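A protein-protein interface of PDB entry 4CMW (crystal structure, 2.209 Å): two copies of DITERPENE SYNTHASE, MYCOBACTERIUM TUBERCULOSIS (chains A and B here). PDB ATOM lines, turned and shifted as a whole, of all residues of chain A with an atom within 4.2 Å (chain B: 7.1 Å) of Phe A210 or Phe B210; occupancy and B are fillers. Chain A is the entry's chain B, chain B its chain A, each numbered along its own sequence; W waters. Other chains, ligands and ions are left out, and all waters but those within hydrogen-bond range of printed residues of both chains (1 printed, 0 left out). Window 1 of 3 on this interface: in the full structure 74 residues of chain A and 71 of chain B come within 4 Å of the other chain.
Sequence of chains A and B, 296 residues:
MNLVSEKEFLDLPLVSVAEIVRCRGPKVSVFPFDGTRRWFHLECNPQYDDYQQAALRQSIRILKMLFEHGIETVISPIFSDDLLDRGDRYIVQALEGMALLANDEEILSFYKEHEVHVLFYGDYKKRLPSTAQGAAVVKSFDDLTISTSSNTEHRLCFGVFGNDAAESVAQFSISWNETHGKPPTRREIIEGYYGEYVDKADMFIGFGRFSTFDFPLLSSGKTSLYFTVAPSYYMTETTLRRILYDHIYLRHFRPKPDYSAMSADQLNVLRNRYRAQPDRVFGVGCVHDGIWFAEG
Phe A210 touches Arg B251, and with the chains exchanged Arg A251 touches Phe B210.
Ser A211 touches Thr B223, and with the chains exchanged Thr A223 touches Ser B211.
Arg A251 touches Gly B283, and with the chains exchanged Gly A283 touches Arg B251.
Phe B282 touches its own counterpart, Phe A282.
Of the printed residues of chain B, Phe A210 touches Phe B210, Thr B223, Leu B225, Arg B251 and Phe B282.
Printed residues of chain B within 4 Å of Ser A211: Gly B221 (3.4 Å), Thr B223 (3.9 Å) and Leu B225 (3.7 Å).
Printed residues of chain B within 4 Å of Phe A227: Val B281 and Phe B282.
Phe B207 touches none of the printed residues of chain A.
Of the printed residues of chain A, Phe B210 touches Phe A210 (3.8 Å), Ser A224 (3.98 Å), Leu A225 (3.0 Å), Arg A251 (2.9 Å) and Phe A282 (3.5 Å).
Ser B224 touches none of the printed residues of chain A.
The nearest printed residue of chain B that does not touch Phe A210 is Ser B224 (4.02 Å).
The nearest printed residue of chain A that does not touch Phe B210 is Thr A223 (4.01 Å).
Among the printed residues, pairs that only touch across the chains: Gly A283 with Tyr B226 (3.2 Å), Phe A282 with Tyr B226 (3.3 Å), Ser A211 with Gly B221 (3.4 Å), Phe A282 with Ala B294 (3.5 Å), Phe A282 with Phe B282 (3.5 Å), Phe A282 with Phe B210 (3.5 Å), Phe A282 with Glu B295 (3.6 Å), Phe A210 with Phe B282 (3.6 Å), Leu A225 with Ser B211 (3.6 Å), Ala A294 with Phe B282 (3.6 Å), Arg A251 with Trp B292 (3.6 Å), Phe A227 with Val B281 (3.7 Å), Ser A211 with Leu B225 (3.7 Å), Thr A223 with Ser B211 (3.7 Å), Phe A210 with Phe B210 (3.8 Å), Ser A211 with Thr B223 (3.9 Å), Phe A210 with Thr B223 (3.9 Å), Leu A225 with Thr B212 (3.9 Å), Leu A225 with Gly B283 (3.9 Å), Gly A283 with Leu B225 (3.98 Å) and Ser A224 with Phe B210 (3.98 Å).
O of Leu B225 is in hydrogen-bond range of NH2 of Arg B251 (3.0 Å).
The backbone carbonyl oxygen (O) of Leu A225 is in hydrogen-bond range of the guanidinium group (NH2) of Arg A251 (2.9 Å).
The backbone NH of Glu B295 is in hydrogen-bond range of the backbone carbonyl oxygen of Val B284 (3.1 Å).
Water W1 lies within hydrogen-bond range of O of Thr A223 (2.6 Å) and N of Thr B212 (3.0 Å).
O of Phe B282 is in hydrogen-bond range of N of Phe A227 (2.8 Å).
N of Leu B225 lies within hydrogen-bond range of O of Phe A210, at 3.1 Å.
The backbone NH of Phe B227 lies within hydrogen-bond range of the backbone carbonyl oxygen of Phe A282.
NH2 of Arg A251 is in hydrogen-bond range of O of Gly B283, at 2.9 Å.
NH1 of Arg B251 is in hydrogen-bond range of O of Phe A210.
The backbone carbonyl oxygen (O) of Gly A283 lies within hydrogen-bond range of the guanidinium group (NH2) of Arg B251 (2.8 Å).
N of Leu A225 lies within hydrogen-bond range of O of Phe B210, at 3.0 Å.
The guanidinium group of Arg A209 is in hydrogen-bond range of the backbone carbonyl oxygen of Arg B251, 2.7 Å away.
The backbone carbonyl oxygen (O) of Phe B210 is in hydrogen-bond range of the guanidinium group (NH1) of Arg A251 (2.9 Å).
O of Arg A251 lies within hydrogen-bond range of NH1 of Arg B209 (2.7 Å).
Printed residues of chain B that touch a printed residue of chain A: Arg B209, Phe B210, Ser B211, Thr B212, Gly B221, Thr B223, Leu B225, Tyr B226, Phe B227, Arg B251, Val B281, Phe B282, Gly B283, Trp B292, Ala B294 and Glu B295.
Hydrophobic or aromatic side chains of chain B within 4 Å of the printed part of chain A: Phe B210, Leu B225, Tyr B226, Val B281, Phe B282, Trp B292 and Ala B294.
Printed residues of chain A that touch a printed residue of chain B: Arg A209, Phe A210, Ser A211, Thr A223, Ser A224, Leu A225, Phe A227, Arg A251, Phe A282, Gly A283 and Ala A294.
Hydrophobic or aromatic side chains of chain A within 4 Å of the printed part of chain B: Phe A210, Leu A225, Phe A282 and Ala A294.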
ATOM      1  N   GLY A 208      14.136  -4.421  21.543  1.00  0.00           N
ATOM      2  CA  GLY A 208      15.396  -3.808  21.142  1.00  0.00           C
ATOM      3  C   GLY A 208      15.391  -3.232  19.728  1.00  0.00           C
ATOM      4  O   GLY A 208      14.508  -2.434  19.374  1.00  0.00           O
ATOM      5  N   ARG A 209      16.390  -3.612  18.932  1.00  0.00           N
ATOM      6  CA  ARG A 209      16.478  -3.198  17.531  1.00  0.00           C
ATOM      7  C   ARG A 209      15.182  -3.520  16.801  1.00  0.00           C
ATOM      8  O   ARG A 209      14.631  -4.611  16.965  1.00  0.00           O
ATOM      9  CB  ARG A 209      17.673  -3.876  16.840  1.00  0.00           C
ATOM     10  CG  ARG A 209      19.046  -3.281  17.263  1.00  0.00           C
ATOM     11  CD  ARG A 209      20.217  -4.152  16.798  1.00  0.00           C
ATOM     12  NE  ARG A 209      20.155  -5.455  17.445  1.00  0.00           N
ATOM     13  CZ  ARG A 209      20.915  -6.499  17.142  1.00  0.00           C
ATOM     14  NH1 ARG A 209      21.820  -6.418  16.179  1.00  0.00           N
ATOM     15  NH2 ARG A 209      20.755  -7.631  17.811  1.00  0.00           N
ATOM     16  N   PHE A 210      14.679  -2.564  16.019  1.00  0.00           N
ATOM     17  CA  PHE A 210      13.382  -2.755  15.383  1.00  0.00           C
ATOM     18  C   PHE A 210      13.574  -3.754  14.254  1.00  0.00           C
ATOM     19  O   PHE A 210      14.241  -3.465  13.269  1.00  0.00           O
ATOM     20  CB  PHE A 210      12.784  -1.445  14.834  1.00  0.00           C
ATOM     21  CG  PHE A 210      12.422  -0.423  15.892  1.00  0.00           C
ATOM     22  CD1 PHE A 210      12.729  -0.620  17.230  1.00  0.00           C
ATOM     23  CD2 PHE A 210      11.744   0.739  15.531  1.00  0.00           C
ATOM     24  CE1 PHE A 210      12.380   0.328  18.187  1.00  0.00           C
ATOM     25  CE2 PHE A 210      11.381   1.689  16.479  1.00  0.00           C
ATOM     26  CZ  PHE A 210      11.717   1.492  17.810  1.00  0.00           C
ATOM     27  N   SER A 211      12.983  -4.930  14.401  1.00  0.00           N
ATOM     28  CA  SER A 211      13.077  -5.947  13.364  1.00  0.00           C
ATOM     29  C   SER A 211      12.029  -6.993  13.651  1.00  0.00           C
ATOM     30  O   SER A 211      11.639  -7.165  14.803  1.00  0.00           O
ATOM     31  CB  SER A 211      14.455  -6.597  13.385  1.00  0.00           C
ATOM     32  OG  SER A 211      14.627  -7.341  14.567  1.00  0.00           O
ATOM     33  N   THR A 223      -0.539  -5.924  10.255  1.00  0.00           N
ATOM     34  CA  THR A 223       0.129  -6.401  11.471  1.00  0.00           C
ATOM     35  C   THR A 223       0.752  -5.245  12.259  1.00  0.00           C
ATOM     36  O   THR A 223       1.739  -4.668  11.811  1.00  0.00           O
ATOM     37  CB  THR A 223       1.241  -7.387  11.126  1.00  0.00           C
ATOM     38  OG1 THR A 223       0.716  -8.398  10.267  1.00  0.00           O
ATOM     39  CG2 THR A 223       1.785  -8.010  12.377  1.00  0.00           C
ATOM     40  N   SER A 224       0.188  -4.918  13.421  1.00  0.00           N
ATOM     41  CA  SER A 224       0.745  -3.889  14.306  1.00  0.00           C
ATOM     42  C   SER A 224       2.090  -4.301  14.900  1.00  0.00           C
ATOM     43  O   SER A 224       2.207  -5.370  15.484  1.00  0.00           O
ATOM     44  CB  SER A 224      -0.200  -3.629  15.483  1.00  0.00           C
ATOM     45  OG  SER A 224      -1.465  -3.216  15.051  1.00  0.00           O
ATOM     46  N   LEU A 225       3.091  -3.437  14.800  1.00  0.00           N
ATOM     47  CA  LEU A 225       4.411  -3.748  15.340  1.00  0.00           C
ATOM     48  C   LEU A 225       4.696  -2.948  16.612  1.00  0.00           C
ATOM     49  O   LEU A 225       4.370  -1.768  16.688  1.00  0.00           O
ATOM     50  CB  LEU A 225       5.483  -3.469  14.290  1.00  0.00           C
ATOM     51  CG  LEU A 225       5.252  -4.116  12.926  1.00  0.00           C
ATOM     52  CD1 LEU A 225       6.410  -3.733  11.991  1.00  0.00           C
ATOM     53  CD2 LEU A 225       5.142  -5.633  13.051  1.00  0.00           C
ATOM     54  N   PHE A 227       7.848  -2.656  19.927  1.00  0.00           N
ATOM     55  CA  PHE A 227       9.186  -3.062  20.329  1.00  0.00           C
ATOM     56  C   PHE A 227       9.450  -2.645  21.760  1.00  0.00           C
ATOM     57  O   PHE A 227       9.472  -1.450  22.064  1.00  0.00           O
ATOM     58  CB  PHE A 227      10.234  -2.492  19.361  1.00  0.00           C
ATOM     59  CG  PHE A 227       9.982  -2.875  17.934  1.00  0.00           C
ATOM     60  CD1 PHE A 227      10.295  -4.154  17.479  1.00  0.00           C
ATOM     61  CD2 PHE A 227       9.397  -1.976  17.047  1.00  0.00           C
ATOM     62  CE1 PHE A 227      10.037  -4.528  16.155  1.00  0.00           C
ATOM     63  CE2 PHE A 227       9.135  -2.342  15.733  1.00  0.00           C
ATOM     64  CZ  PHE A 227       9.461  -3.621  15.285  1.00  0.00           C
ATOM     65  N   ARG A 251      -4.851   2.130  16.452  1.00  0.00           N
ATOM     66  CA  ARG A 251      -4.257   1.807  15.151  1.00  0.00           C
ATOM     67  C   ARG A 251      -5.221   1.960  13.968  1.00  0.00           C
ATOM     68  O   ARG A 251      -4.809   2.334  12.865  1.00  0.00           O
ATOM     69  CB  ARG A 251      -3.638   0.409  15.153  1.00  0.00           C
ATOM     70  CG  ARG A 251      -2.327   0.313  15.922  1.00  0.00           C
ATOM     71  CD  ARG A 251      -1.215   1.201  15.341  1.00  0.00           C
ATOM     72  NE  ARG A 251       0.051   0.968  16.042  1.00  0.00           N
ATOM     73  CZ  ARG A 251       1.075   0.270  15.563  1.00  0.00           C
ATOM     74  NH1 ARG A 251       1.023  -0.244  14.341  1.00  0.00           N
ATOM     75  NH2 ARG A 251       2.176   0.122  16.294  1.00  0.00           N
ATOM     76  N   PHE A 282      11.684   6.911  14.362  1.00  0.00           N
ATOM     77  CA  PHE A 282      11.771   5.848  15.353  1.00  0.00           C
ATOM     78  C   PHE A 282      12.544   4.676  14.760  1.00  0.00           C
ATOM     79  O   PHE A 282      12.341   4.300  13.601  1.00  0.00           O
ATOM     80  CB  PHE A 282      10.374   5.422  15.845  1.00  0.00           C
ATOM     81  CG  PHE A 282       9.725   6.420  16.776  1.00  0.00           C
ATOM     82  CD1 PHE A 282      10.002   6.404  18.137  1.00  0.00           C
ATOM     83  CD2 PHE A 282       8.855   7.387  16.291  1.00  0.00           C
ATOM     84  CE1 PHE A 282       9.414   7.330  19.004  1.00  0.00           C
ATOM     85  CE2 PHE A 282       8.266   8.315  17.146  1.00  0.00           C
ATOM     86  CZ  PHE A 282       8.544   8.289  18.508  1.00  0.00           C
ATOM     87  N   GLY A 283      13.463   4.125  15.541  1.00  0.00           N
ATOM     88  CA  GLY A 283      14.291   3.030  15.062  1.00  0.00           C
ATOM     89  C   GLY A 283      15.732   3.470  14.884  1.00  0.00           C
ATOM     90  O   GLY A 283      16.627   2.645  14.704  1.00  0.00           O
ATOM     91  N   ALA A 294      16.886   2.213  21.278  1.00  0.00           N
ATOM     92  CA  ALA A 294      16.111   3.127  20.444  1.00  0.00           C
ATOM     93  C   ALA A 294      16.059   4.485  21.126  1.00  0.00           C
ATOM     94  O   ALA A 294      15.870   4.567  22.340  1.00  0.00           O
ATOM     95  CB  ALA A 294      14.678   2.576  20.194  1.00  0.00           C
ATOM     96  N   PHE B 207       6.356   4.918   7.779  1.00  0.00           N
ATOM     97  CA  PHE B 207       5.844   6.213   8.208  1.00  0.00           C
ATOM     98  C   PHE B 207       4.743   5.972   9.215  1.00  0.00           C
ATOM     99  O   PHE B 207       3.925   5.096   9.017  1.00  0.00           O
ATOM    100  CB  PHE B 207       5.280   6.990   7.002  1.00  0.00           C
ATOM    101  CG  PHE B 207       4.153   7.931   7.361  1.00  0.00           C
ATOM    102  CD1 PHE B 207       4.407   9.115   8.024  1.00  0.00           C
ATOM    103  CD2 PHE B 207       2.832   7.606   7.069  1.00  0.00           C
ATOM    104  CE1 PHE B 207       3.368   9.976   8.376  1.00  0.00           C
ATOM    105  CE2 PHE B 207       1.786   8.458   7.419  1.00  0.00           C
ATOM    106  CZ  PHE B 207       2.056   9.648   8.068  1.00  0.00           C
ATOM    107  N   GLY B 208       4.700   6.761  10.282  1.00  0.00           N
ATOM    108  CA  GLY B 208       3.594   6.676  11.231  1.00  0.00           C
ATOM    109  C   GLY B 208       3.483   5.369  12.009  1.00  0.00           C
ATOM    110  O   GLY B 208       4.432   4.935  12.657  1.00  0.00           O
ATOM    111  N   ARG B 209       2.307   4.757  11.951  1.00  0.00           N
ATOM    112  CA  ARG B 209       2.033   3.480  12.613  1.00  0.00           C
ATOM    113  C   ARG B 209       3.091   2.455  12.218  1.00  0.00           C
ATOM    114  O   ARG B 209       3.443   2.354  11.040  1.00  0.00           O
ATOM    115  CB  ARG B 209       0.649   2.973  12.224  1.00  0.00           C
ATOM    116  CG  ARG B 209      -0.498   3.792  12.808  1.00  0.00           C
ATOM    117  CD  ARG B 209      -1.851   3.436  12.170  1.00  0.00           C
ATOM    118  NE  ARG B 209      -1.857   3.739  10.743  1.00  0.00           N
ATOM    119  CZ  ARG B 209      -2.820   3.396   9.893  1.00  0.00           C
ATOM    120  NH1 ARG B 209      -3.887   2.732  10.313  1.00  0.00           N
ATOM    121  NH2 ARG B 209      -2.712   3.723   8.611  1.00  0.00           N
ATOM    122  N   PHE B 210       3.618   1.722  13.197  1.00  0.00           N
ATOM    123  CA  PHE B 210       4.714   0.809  12.905  1.00  0.00           C
ATOM    124  C   PHE B 210       4.107  -0.403  12.223  1.00  0.00           C
ATOM    125  O   PHE B 210       3.342  -1.141  12.836  1.00  0.00           O
ATOM    126  CB  PHE B 210       5.498   0.358  14.153  1.00  0.00           C
ATOM    127  CG  PHE B 210       6.184   1.475  14.918  1.00  0.00           C
ATOM    128  CD1 PHE B 210       6.026   2.802  14.561  1.00  0.00           C
ATOM    129  CD2 PHE B 210       6.970   1.177  16.041  1.00  0.00           C
ATOM    130  CE1 PHE B 210       6.648   3.817  15.289  1.00  0.00           C
ATOM    131  CE2 PHE B 210       7.598   2.188  16.771  1.00  0.00           C
ATOM    132  CZ  PHE B 210       7.437   3.506  16.397  1.00  0.00           C
ATOM    133  N   SER B 211       4.449  -0.594  10.950  1.00  0.00           N
ATOM    134  CA  SER B 211       3.998  -1.752  10.193  1.00  0.00           C
ATOM    135  C   SER B 211       4.849  -1.804   8.953  1.00  0.00           C
ATOM    136  O   SER B 211       5.348  -0.771   8.521  1.00  0.00           O
ATOM    137  CB  SER B 211       2.527  -1.614   9.789  1.00  0.00           C
ATOM    138  OG  SER B 211       2.369  -0.582   8.832  1.00  0.00           O
ATOM    139  N   THR B 212       5.028  -2.999   8.395  1.00  0.00           N
ATOM    140  CA  THR B 212       5.722  -3.165   7.112  1.00  0.00           C
ATOM    141  C   THR B 212       4.843  -3.991   6.187  1.00  0.00           C
ATOM    142  O   THR B 212       3.920  -4.676   6.637  1.00  0.00           O
ATOM    143  CB  THR B 212       7.079  -3.891   7.263  1.00  0.00           C
ATOM    144  OG1 THR B 212       6.843  -5.248   7.670  1.00  0.00           O
ATOM    145  CG2 THR B 212       7.946  -3.200   8.304  1.00  0.00           C
ATOM    146  N   GLY B 221      15.121 -11.017   9.738  1.00  0.00           N
ATOM    147  CA  GLY B 221      15.427 -10.423  11.021  1.00  0.00           C
ATOM    148  C   GLY B 221      16.551  -9.420  10.909  1.00  0.00           C
ATOM    149  O   GLY B 221      16.762  -8.619  11.813  1.00  0.00           O
ATOM    150  N   LYS B 222      17.269  -9.454   9.792  1.00  0.00           N
ATOM    151  CA  LYS B 222      18.357  -8.519   9.581  1.00  0.00           C
ATOM    152  C   LYS B 222      17.911  -7.272   8.846  1.00  0.00           C
ATOM    153  O   LYS B 222      18.697  -6.356   8.651  1.00  0.00           O
ATOM    154  CB  LYS B 222      19.511  -9.195   8.850  1.00  0.00           C
ATOM    155  CG  LYS B 222      20.242 -10.216   9.718  1.00  0.00           C
ATOM    156  CD  LYS B 222      21.358 -10.900   8.939  1.00  0.00           C
ATOM    157  CE  LYS B 222      22.164 -11.845   9.821  1.00  0.00           C
ATOM    158  NZ  LYS B 222      22.973 -11.093  10.827  1.00  0.00           N
ATOM    159  N   THR B 223      16.644  -7.231   8.445  1.00  0.00           N
ATOM    160  CA  THR B 223      16.090  -6.015   7.871  1.00  0.00           C
ATOM    161  C   THR B 223      15.863  -4.979   8.984  1.00  0.00           C
ATOM    162  O   THR B 223      14.982  -5.158   9.831  1.00  0.00           O
ATOM    163  CB  THR B 223      14.751  -6.286   7.129  1.00  0.00           C
ATOM    164  OG1 THR B 223      14.916  -7.357   6.177  1.00  0.00           O
ATOM    165  CG2 THR B 223      14.297  -5.020   6.405  1.00  0.00           C
ATOM    166  N   SER B 224      16.668  -3.914   8.993  1.00  0.00           N
ATOM    167  CA  SER B 224      16.486  -2.809   9.941  1.00  0.00           C
ATOM    168  C   SER B 224      15.195  -2.058   9.630  1.00  0.00           C
ATOM    169  O   SER B 224      14.964  -1.676   8.489  1.00  0.00           O
ATOM    170  CB  SER B 224      17.653  -1.824   9.854  1.00  0.00           C
ATOM    171  OG  SER B 224      18.878  -2.470  10.148  1.00  0.00           O
ATOM    172  N   LEU B 225      14.351  -1.847  10.634  1.00  0.00           N
ATOM    173  CA  LEU B 225      13.087  -1.149  10.399  1.00  0.00           C
ATOM    174  C   LEU B 225      13.133   0.253  11.000  1.00  0.00           C
ATOM    175  O   LEU B 225      13.550   0.421  12.156  1.00  0.00           O
ATOM    176  CB  LEU B 225      11.920  -1.941  11.009  1.00  0.00           C
ATOM    177  CG  LEU B 225      11.824  -3.423  10.634  1.00  0.00           C
ATOM    178  CD1 LEU B 225      10.624  -4.097  11.334  1.00  0.00           C
ATOM    179  CD2 LEU B 225      11.712  -3.577   9.119  1.00  0.00           C
ATOM    180  N   TYR B 226      12.675   1.246  10.233  1.00  0.00           N
ATOM    181  CA  TYR B 226      12.587   2.623  10.720  1.00  0.00           C
ATOM    182  C   TYR B 226      11.194   3.160  10.459  1.00  0.00           C
ATOM    183  O   TYR B 226      10.547   2.715   9.524  1.00  0.00           O
ATOM    184  CB  TYR B 226      13.616   3.510  10.015  1.00  0.00           C
ATOM    185  CG  TYR B 226      15.007   3.005  10.210  1.00  0.00           C
ATOM    186  CD1 TYR B 226      15.750   3.373  11.337  1.00  0.00           C
ATOM    187  CD2 TYR B 226      15.564   2.106   9.307  1.00  0.00           C
ATOM    188  CE1 TYR B 226      17.021   2.882  11.537  1.00  0.00           C
ATOM    189  CE2 TYR B 226      16.835   1.620   9.493  1.00  0.00           C
ATOM    190  CZ  TYR B 226      17.560   2.005  10.608  1.00  0.00           C
ATOM    191  OH  TYR B 226      18.817   1.493  10.781  1.00  0.00           O
ATOM    192  N   PHE B 227      10.719   4.093  11.291  1.00  0.00           N
ATOM    193  CA  PHE B 227       9.409   4.718  11.050  1.00  0.00           C
ATOM    194  C   PHE B 227       9.467   6.213  11.263  1.00  0.00           C
ATOM    195  O   PHE B 227       9.632   6.683  12.389  1.00  0.00           O
ATOM    196  CB  PHE B 227       8.332   4.069  11.922  1.00  0.00           C
ATOM    197  CG  PHE B 227       8.276   2.586  11.762  1.00  0.00           C
ATOM    198  CD1 PHE B 227       7.657   2.015  10.649  1.00  0.00           C
ATOM    199  CD2 PHE B 227       8.903   1.758  12.682  1.00  0.00           C
ATOM    200  CE1 PHE B 227       7.631   0.636  10.481  1.00  0.00           C
ATOM    201  CE2 PHE B 227       8.892   0.384  12.518  1.00  0.00           C
ATOM    202  CZ  PHE B 227       8.248  -0.178  11.414  1.00  0.00           C
ATOM    203  N   THR B 228       9.337   6.964  10.171  1.00  0.00           N
ATOM    204  CA  THR B 228       9.405   8.419  10.271  1.00  0.00           C
ATOM    205  C   THR B 228       8.138   8.954  10.922  1.00  0.00           C
ATOM    206  O   THR B 228       7.076   8.330  10.846  1.00  0.00           O
ATOM    207  CB  THR B 228       9.607   9.094   8.890  1.00  0.00           C
ATOM    208  OG1 THR B 228       8.501   8.775   8.037  1.00  0.00           O
ATOM    209  CG2 THR B 228      10.908   8.607   8.229  1.00  0.00           C
ATOM    210  N   ARG B 251      23.380  -0.768  14.278  1.00  0.00           N
ATOM    211  CA  ARG B 251      22.556  -1.974  14.312  1.00  0.00           C
ATOM    212  C   ARG B 251      23.375  -3.254  14.477  1.00  0.00           C
ATOM    213  O   ARG B 251      22.932  -4.207  15.100  1.00  0.00           O
ATOM    214  CB  ARG B 251      21.673  -2.072  13.067  1.00  0.00           C
ATOM    215  CG  ARG B 251      20.507  -1.074  13.016  1.00  0.00           C
ATOM    216  CD  ARG B 251      19.506  -1.270  14.144  1.00  0.00           C
ATOM    217  NE  ARG B 251      18.337  -0.391  14.031  1.00  0.00           N
ATOM    218  CZ  ARG B 251      17.115  -0.776  13.625  1.00  0.00           C
ATOM    219  NH1 ARG B 251      16.870  -2.037  13.281  1.00  0.00           N
ATOM    220  NH2 ARG B 251      16.122   0.104  13.585  1.00  0.00           N
ATOM    221  N   VAL B 281       7.600   0.960  25.755  1.00  0.00           N
ATOM    222  CA  VAL B 281       7.330   0.214  24.526  1.00  0.00           C
ATOM    223  C   VAL B 281       7.175   1.148  23.333  1.00  0.00           C
ATOM    224  O   VAL B 281       6.321   2.027  23.309  1.00  0.00           O
ATOM    225  CB  VAL B 281       6.056  -0.640  24.609  1.00  0.00           C
ATOM    226  CG1 VAL B 281       5.896  -1.454  23.344  1.00  0.00           C
ATOM    227  CG2 VAL B 281       6.107  -1.550  25.788  1.00  0.00           C
ATOM    228  N   PHE B 282       8.021   0.958  22.339  1.00  0.00           N
ATOM    229  CA  PHE B 282       7.877   1.721  21.109  1.00  0.00           C
ATOM    230  C   PHE B 282       6.781   1.116  20.224  1.00  0.00           C
ATOM    231  O   PHE B 282       6.713  -0.102  20.055  1.00  0.00           O
ATOM    232  CB  PHE B 282       9.222   1.805  20.385  1.00  0.00           C
ATOM    233  CG  PHE B 282      10.196   2.723  21.061  1.00  0.00           C
ATOM    234  CD1 PHE B 282      10.167   4.086  20.816  1.00  0.00           C
ATOM    235  CD2 PHE B 282      11.118   2.234  21.966  1.00  0.00           C
ATOM    236  CE1 PHE B 282      11.054   4.951  21.450  1.00  0.00           C
ATOM    237  CE2 PHE B 282      12.016   3.093  22.597  1.00  0.00           C
ATOM    238  CZ  PHE B 282      11.976   4.455  22.344  1.00  0.00           C
ATOM    239  N   GLY B 283       5.932   1.972  19.660  1.00  0.00           N
ATOM    240  CA  GLY B 283       4.846   1.524  18.802  1.00  0.00           C
ATOM    241  C   GLY B 283       3.475   1.777  19.409  1.00  0.00           C
ATOM    242  O   GLY B 283       2.446   1.691  18.736  1.00  0.00           O
ATOM    243  N   VAL B 284       3.460   2.074  20.699  1.00  0.00           N
ATOM    244  CA  VAL B 284       2.238   2.498  21.349  1.00  0.00           C
ATOM    245  C   VAL B 284       2.056   3.985  21.041  1.00  0.00           C
ATOM    246  O   VAL B 284       2.966   4.792  21.238  1.00  0.00           O
ATOM    247  CB  VAL B 284       2.285   2.223  22.872  1.00  0.00           C
ATOM    248  CG1 VAL B 284       1.143   2.930  23.590  1.00  0.00           C
ATOM    249  CG2 VAL B 284       2.235   0.710  23.136  1.00  0.00           C
ATOM    250  N   TRP B 292      -2.903   9.346  14.363  1.00  0.00           N
ATOM    251  CA  TRP B 292      -2.074   8.539  15.243  1.00  0.00           C
ATOM    252  C   TRP B 292      -0.629   9.031  15.189  1.00  0.00           C
ATOM    253  O   TRP B 292      -0.099   9.291  14.120  1.00  0.00           O
ATOM    254  CB  TRP B 292      -2.132   7.089  14.774  1.00  0.00           C
ATOM    255  CG  TRP B 292      -1.428   6.084  15.627  1.00  0.00           C
ATOM    256  CD1 TRP B 292      -1.997   5.250  16.544  1.00  0.00           C
ATOM    257  CD2 TRP B 292      -0.025   5.789  15.632  1.00  0.00           C
ATOM    258  NE1 TRP B 292      -1.038   4.450  17.116  1.00  0.00           N
ATOM    259  CE2 TRP B 292       0.182   4.758  16.568  1.00  0.00           C
ATOM    260  CE3 TRP B 292       1.079   6.290  14.925  1.00  0.00           C
ATOM    261  CZ2 TRP B 292       1.444   4.222  16.823  1.00  0.00           C
ATOM    262  CZ3 TRP B 292       2.333   5.761  15.180  1.00  0.00           C
ATOM    263  CH2 TRP B 292       2.506   4.736  16.120  1.00  0.00           C
ATOM    264  N   PHE B 293      -0.011   9.156  16.352  1.00  0.00           N
ATOM    265  CA  PHE B 293       1.399   9.519  16.499  1.00  0.00           C
ATOM    266  C   PHE B 293       2.046   8.558  17.494  1.00  0.00           C
ATOM    267  O   PHE B 293       1.473   8.319  18.560  1.00  0.00           O
ATOM    268  CB  PHE B 293       1.538  10.927  17.086  1.00  0.00           C
ATOM    269  CG  PHE B 293       1.242  12.036  16.119  1.00  0.00           C
ATOM    270  CD1 PHE B 293       2.250  12.589  15.343  1.00  0.00           C
ATOM    271  CD2 PHE B 293      -0.035  12.548  16.006  1.00  0.00           C
ATOM    272  CE1 PHE B 293       1.984  13.617  14.458  1.00  0.00           C
ATOM    273  CE2 PHE B 293      -0.303  13.573  15.123  1.00  0.00           C
ATOM    274  CZ  PHE B 293       0.704  14.110  14.352  1.00  0.00           C
ATOM    275  N   ALA B 294       3.234   8.054  17.188  1.00  0.00           N
ATOM    276  CA  ALA B 294       3.964   7.249  18.151  1.00  0.00           C
ATOM    277  C   ALA B 294       4.374   8.105  19.360  1.00  0.00           C
ATOM    278  O   ALA B 294       4.727   9.270  19.208  1.00  0.00           O
ATOM    279  CB  ALA B 294       5.202   6.628  17.497  1.00  0.00           C
ATOM    280  N   GLU B 295       4.288   7.529  20.556  1.00  0.00           N
ATOM    281  CA  GLU B 295       4.773   8.171  21.777  1.00  0.00           C
ATOM    282  C   GLU B 295       6.260   7.905  22.001  1.00  0.00           C
ATOM    283  O   GLU B 295       6.827   6.987  21.414  1.00  0.00           O
ATOM    284  CB  GLU B 295       3.987   7.649  22.979  1.00  0.00           C
ATOM    285  CG  GLU B 295       2.543   8.126  23.013  1.00  0.00           C
ATOM    286  CD  GLU B 295       1.775   7.580  24.194  1.00  0.00           C
ATOM    287  OE1 GLU B 295       2.121   6.476  24.676  1.00  0.00           O
ATOM    288  OE2 GLU B 295       0.822   8.254  24.633  1.00  0.00           O
HETATM  289  O   HOH W   1       3.100  -4.943   9.618  1.00  0.00           O
